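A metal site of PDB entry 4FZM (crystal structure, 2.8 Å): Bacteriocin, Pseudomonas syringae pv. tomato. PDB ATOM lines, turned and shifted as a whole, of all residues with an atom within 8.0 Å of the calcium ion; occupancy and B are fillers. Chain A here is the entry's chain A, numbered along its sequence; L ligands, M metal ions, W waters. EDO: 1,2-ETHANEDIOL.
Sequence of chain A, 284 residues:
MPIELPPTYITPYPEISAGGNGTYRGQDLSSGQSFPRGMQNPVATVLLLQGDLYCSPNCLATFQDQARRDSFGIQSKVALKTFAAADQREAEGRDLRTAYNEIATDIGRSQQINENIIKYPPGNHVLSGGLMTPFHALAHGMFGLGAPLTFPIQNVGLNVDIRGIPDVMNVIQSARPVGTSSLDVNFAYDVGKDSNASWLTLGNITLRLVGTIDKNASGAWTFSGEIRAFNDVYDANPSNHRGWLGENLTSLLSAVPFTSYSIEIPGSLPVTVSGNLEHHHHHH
The backbone carbonyl oxygen of Asp 232 is in hydrogen-bond range of the backbone NH of Ile 263 (2.8 Å).
Three residues have an atom within 4 Å of the calcium ion: Leu 202, Asn 204 and Asp 232. The nearest printed residue that does not touch the calcium ion is Gly 203 (4.1 Å).
The backbone carbonyl oxygen (O) of Leu 202 binds the calcium ion, 2.3 Å away. The calcium ion is bound by O1 of the ligand (2.4 Å). The side-chain carboxylate (OD2) of Asp 232 binds the calcium ion (2.4 Å). The calcium ion is bound by O of Asn 204 (2.5 Å). The calcium ion is bound by O2 of the ligand (2.5 Å). The calcium ion is bound by OD1 of Asp 232, at 2.6 Å. Water W1 binds the calcium ion.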
ATOM      1  N   TYR A 189      -6.150 -24.029  12.890  1.00  0.00           N
ATOM      2  CA  TYR A 189      -7.316 -24.820  13.115  1.00  0.00           C
ATOM      3  C   TYR A 189      -7.630 -25.578  11.876  1.00  0.00           C
ATOM      4  O   TYR A 189      -7.672 -25.031  10.810  1.00  0.00           O
ATOM      5  CB  TYR A 189      -8.501 -23.962  13.430  1.00  0.00           C
ATOM      6  CG  TYR A 189      -9.742 -24.731  13.923  1.00  0.00           C
ATOM      7  CD1 TYR A 189      -9.927 -24.971  15.268  1.00  0.00           C
ATOM      8  CD2 TYR A 189     -10.748 -25.108  13.049  1.00  0.00           C
ATOM      9  CE1 TYR A 189     -11.045 -25.594  15.709  1.00  0.00           C
ATOM     10  CE2 TYR A 189     -11.908 -25.699  13.501  1.00  0.00           C
ATOM     11  CZ  TYR A 189     -12.037 -25.975  14.831  1.00  0.00           C
ATOM     12  OH  TYR A 189     -13.188 -26.619  15.349  1.00  0.00           O
ATOM     13  N   VAL A 191      -9.950 -27.121   9.764  1.00  0.00           N
ATOM     14  CA  VAL A 191     -11.413 -27.071   9.567  1.00  0.00           C
ATOM     15  C   VAL A 191     -11.975 -28.469   9.504  1.00  0.00           C
ATOM     16  O   VAL A 191     -13.183 -28.707   9.631  1.00  0.00           O
ATOM     17  CB  VAL A 191     -11.754 -26.414   8.253  1.00  0.00           C
ATOM     18  CG1 VAL A 191     -13.194 -26.654   7.887  1.00  0.00           C
ATOM     19  CG2 VAL A 191     -11.466 -24.919   8.341  1.00  0.00           C
ATOM     20  N   TRP A 199     -13.045 -28.552   4.725  1.00  0.00           N
ATOM     21  CA  TRP A 199     -11.602 -28.844   4.638  1.00  0.00           C
ATOM     22  C   TRP A 199     -11.110 -28.984   3.218  1.00  0.00           C
ATOM     23  O   TRP A 199     -10.042 -28.472   2.867  1.00  0.00           O
ATOM     24  CB  TRP A 199     -11.254 -30.080   5.447  1.00  0.00           C
ATOM     25  CG  TRP A 199      -9.820 -30.347   5.547  1.00  0.00           C
ATOM     26  CD1 TRP A 199      -8.873 -29.729   6.329  1.00  0.00           C
ATOM     27  CD2 TRP A 199      -9.130 -31.403   4.884  1.00  0.00           C
ATOM     28  NE1 TRP A 199      -7.599 -30.313   6.162  1.00  0.00           N
ATOM     29  CE2 TRP A 199      -7.736 -31.341   5.326  1.00  0.00           C
ATOM     30  CE3 TRP A 199      -9.491 -32.346   3.980  1.00  0.00           C
ATOM     31  CZ2 TRP A 199      -6.826 -32.190   4.841  1.00  0.00           C
ATOM     32  CZ3 TRP A 199      -8.550 -33.208   3.505  1.00  0.00           C
ATOM     33  CH2 TRP A 199      -7.276 -33.140   3.902  1.00  0.00           C
ATOM     34  N   THR A 201     -11.934 -27.339   0.673  1.00  0.00           N
ATOM     35  CA  THR A 201     -11.660 -25.987   0.218  1.00  0.00           C
ATOM     36  C   THR A 201     -10.645 -25.185   1.008  1.00  0.00           C
ATOM     37  O   THR A 201      -9.963 -24.411   0.411  1.00  0.00           O
ATOM     38  CB  THR A 201     -12.942 -25.175   0.198  1.00  0.00           C
ATOM     39  OG1 THR A 201     -13.939 -25.982  -0.489  1.00  0.00           O
ATOM     40  CG2 THR A 201     -12.745 -23.897  -0.442  1.00  0.00           C
ATOM     41  N   LEU A 202     -10.496 -25.365   2.307  1.00  0.00           N
ATOM     42  CA  LEU A 202      -9.712 -24.422   3.108  1.00  0.00           C
ATOM     43  C   LEU A 202      -8.460 -25.070   3.755  1.00  0.00           C
ATOM     44  O   LEU A 202      -7.439 -24.406   4.010  1.00  0.00           O
ATOM     45  CB  LEU A 202     -10.584 -23.910   4.268  1.00  0.00           C
ATOM     46  CG  LEU A 202     -11.686 -22.880   4.046  1.00  0.00           C
ATOM     47  CD1 LEU A 202     -12.508 -22.613   5.299  1.00  0.00           C
ATOM     48  CD2 LEU A 202     -11.175 -21.565   3.454  1.00  0.00           C
ATOM     49  N   GLY A 203      -8.576 -26.340   4.148  1.00  0.00           N
ATOM     50  CA  GLY A 203      -7.490 -26.977   4.862  1.00  0.00           C
ATOM     51  C   GLY A 203      -7.316 -26.391   6.235  1.00  0.00           C
ATOM     52  O   GLY A 203      -8.215 -26.453   7.042  1.00  0.00           O
ATOM     53  N   ASN A 204      -6.172 -25.837   6.572  1.00  0.00           N
ATOM     54  CA  ASN A 204      -6.138 -25.211   7.884  1.00  0.00           C
ATOM     55  C   ASN A 204      -6.373 -23.740   7.695  1.00  0.00           C
ATOM     56  O   ASN A 204      -6.116 -23.173   6.598  1.00  0.00           O
ATOM     57  CB  ASN A 204      -4.829 -25.431   8.613  1.00  0.00           C
ATOM     58  CG  ASN A 204      -4.474 -26.891   8.766  1.00  0.00           C
ATOM     59  OD1 ASN A 204      -5.329 -27.773   8.772  1.00  0.00           O
ATOM     60  ND2 ASN A 204      -3.206 -27.149   8.888  1.00  0.00           N
ATOM     61  N   ILE A 205      -6.880 -23.107   8.725  1.00  0.00           N
ATOM     62  CA  ILE A 205      -7.023 -21.714   8.616  1.00  0.00           C
ATOM     63  C   ILE A 205      -6.462 -21.165   9.870  1.00  0.00           C
ATOM     64  O   ILE A 205      -6.180 -21.938  10.782  1.00  0.00           O
ATOM     65  CB  ILE A 205      -8.478 -21.314   8.428  1.00  0.00           C
ATOM     66  CG1 ILE A 205      -9.340 -21.828   9.572  1.00  0.00           C
ATOM     67  CG2 ILE A 205      -8.976 -21.775   7.071  1.00  0.00           C
ATOM     68  CD1 ILE A 205     -10.787 -21.404   9.348  1.00  0.00           C
ATOM     69  N   THR A 206      -6.299 -19.854   9.963  1.00  0.00           N
ATOM     70  CA  THR A 206      -6.028 -19.300  11.257  1.00  0.00           C
ATOM     71  C   THR A 206      -7.269 -18.616  11.804  1.00  0.00           C
ATOM     72  O   THR A 206      -7.905 -17.819  11.097  1.00  0.00           O
ATOM     73  CB  THR A 206      -4.859 -18.346  11.158  1.00  0.00           C
ATOM     74  OG1 THR A 206      -3.865 -19.032  10.396  1.00  0.00           O
ATOM     75  CG2 THR A 206      -4.331 -18.017  12.513  1.00  0.00           C
ATOM     76  N   PHE A 230      -8.866 -15.358   9.627  1.00  0.00           N
ATOM     77  CA  PHE A 230      -8.028 -14.715   8.647  1.00  0.00           C
ATOM     78  C   PHE A 230      -8.158 -15.317   7.279  1.00  0.00           C
ATOM     79  O   PHE A 230      -8.187 -16.522   7.128  1.00  0.00           O
ATOM     80  CB  PHE A 230      -6.585 -14.736   9.134  1.00  0.00           C
ATOM     81  CG  PHE A 230      -6.386 -13.802  10.270  1.00  0.00           C
ATOM     82  CD1 PHE A 230      -6.865 -12.446  10.163  1.00  0.00           C
ATOM     83  CD2 PHE A 230      -5.859 -14.245  11.466  1.00  0.00           C
ATOM     84  CE1 PHE A 230      -6.794 -11.553  11.216  1.00  0.00           C
ATOM     85  CE2 PHE A 230      -5.749 -13.360  12.529  1.00  0.00           C
ATOM     86  CZ  PHE A 230      -6.225 -12.030  12.400  1.00  0.00           C
ATOM     87  N   ASN A 231      -8.264 -14.473   6.275  1.00  0.00           N
ATOM     88  CA  ASN A 231      -8.164 -14.913   4.891  1.00  0.00           C
ATOM     89  C   ASN A 231      -7.196 -16.074   4.636  1.00  0.00           C
ATOM     90  O   ASN A 231      -6.138 -16.066   5.161  1.00  0.00           O
ATOM     91  CB  ASN A 231      -7.848 -13.713   4.018  1.00  0.00           C
ATOM     92  CG  ASN A 231      -8.835 -12.578   4.279  1.00  0.00           C
ATOM     93  OD1 ASN A 231      -9.844 -12.777   4.963  1.00  0.00           O
ATOM     94  ND2 ASN A 231      -8.526 -11.388   3.809  1.00  0.00           N
ATOM     95  N   ASP A 232      -7.628 -17.086   3.888  1.00  0.00           N
ATOM     96  CA  ASP A 232      -6.808 -18.275   3.527  1.00  0.00           C
ATOM     97  C   ASP A 232      -6.511 -18.180   2.022  1.00  0.00           C
ATOM     98  O   ASP A 232      -7.158 -17.426   1.290  1.00  0.00           O
ATOM     99  CB  ASP A 232      -7.599 -19.582   3.773  1.00  0.00           C
ATOM    100  CG  ASP A 232      -6.702 -20.840   3.948  1.00  0.00           C
ATOM    101  OD1 ASP A 232      -5.812 -20.924   4.862  1.00  0.00           O
ATOM    102  OD2 ASP A 232      -6.925 -21.815   3.185  1.00  0.00           O
ATOM    103  N   VAL A 233      -5.532 -18.946   1.573  1.00  0.00           N
ATOM    104  CA  VAL A 233      -5.132 -18.906   0.166  1.00  0.00           C
ATOM    105  C   VAL A 233      -5.351 -20.246  -0.494  1.00  0.00           C
ATOM    106  O   VAL A 233      -4.650 -21.197  -0.200  1.00  0.00           O
ATOM    107  CB  VAL A 233      -3.615 -18.643   0.007  1.00  0.00           C
ATOM    108  CG1 VAL A 233      -3.107 -19.173  -1.345  1.00  0.00           C
ATOM    109  CG2 VAL A 233      -3.342 -17.196   0.223  1.00  0.00           C
ATOM    110  N   TYR A 234      -6.271 -20.293  -1.429  1.00  0.00           N
ATOM    111  CA  TYR A 234      -6.572 -21.515  -2.189  1.00  0.00           C
ATOM    112  C   TYR A 234      -5.454 -21.744  -3.192  1.00  0.00           C
ATOM    113  O   TYR A 234      -5.267 -20.946  -4.131  1.00  0.00           O
ATOM    114  CB  TYR A 234      -7.885 -21.330  -2.952  1.00  0.00           C
ATOM    115  CG  TYR A 234      -8.409 -22.557  -3.528  1.00  0.00           C
ATOM    116  CD1 TYR A 234      -9.147 -23.367  -2.800  1.00  0.00           C
ATOM    117  CD2 TYR A 234      -8.157 -22.894  -4.801  1.00  0.00           C
ATOM    118  CE1 TYR A 234      -9.659 -24.531  -3.312  1.00  0.00           C
ATOM    119  CE2 TYR A 234      -8.669 -24.040  -5.350  1.00  0.00           C
ATOM    120  CZ  TYR A 234      -9.425 -24.859  -4.599  1.00  0.00           C
ATOM    121  OH  TYR A 234      -9.948 -26.044  -5.083  1.00  0.00           O
ATOM    122  N   ASP A 235      -4.723 -22.832  -2.990  1.00  0.00           N
ATOM    123  CA  ASP A 235      -3.634 -23.186  -3.880  1.00  0.00           C
ATOM    124  C   ASP A 235      -4.268 -24.041  -4.936  1.00  0.00           C
ATOM    125  O   ASP A 235      -4.654 -25.148  -4.690  1.00  0.00           O
ATOM    126  CB  ASP A 235      -2.551 -23.958  -3.151  1.00  0.00           C
ATOM    127  CG  ASP A 235      -1.310 -24.172  -4.003  1.00  0.00           C
ATOM    128  OD1 ASP A 235      -0.215 -24.409  -3.426  1.00  0.00           O
ATOM    129  OD2 ASP A 235      -1.415 -24.108  -5.247  1.00  0.00           O
ATOM    130  N   ILE A 263      -9.128 -16.440  -0.480  1.00  0.00           N
ATOM    131  CA  ILE A 263     -10.460 -16.623   0.091  1.00  0.00           C
ATOM    132  C   ILE A 263     -10.636 -15.774   1.330  1.00  0.00           C
ATOM    133  O   ILE A 263     -10.058 -16.051   2.379  1.00  0.00           O
ATOM    134  CB  ILE A 263     -10.775 -18.065   0.556  1.00  0.00           C
ATOM    135  CG1 ILE A 263     -10.378 -19.111  -0.472  1.00  0.00           C
ATOM    136  CG2 ILE A 263     -12.263 -18.170   0.854  1.00  0.00           C
ATOM    137  CD1 ILE A 263     -11.019 -20.458  -0.254  1.00  0.00           C
HETATM  138  C1  EDO L   1      -2.919 -21.935   2.664  1.00  0.00           C
HETATM  139  O1  EDO L   1      -4.285 -22.399   2.425  1.00  0.00           O
HETATM  140  C2  EDO L   1      -2.733 -21.427   4.081  1.00  0.00           C
HETATM  141  O2  EDO L   1      -3.319 -22.335   5.020  1.00  0.00           O
HETATM  142 CA    CA M   1      -5.411 -23.386   4.254  1.00  0.00          CA
HETATM  143  O   HOH W   1      -3.274 -25.021   4.852  1.00  0.00           O
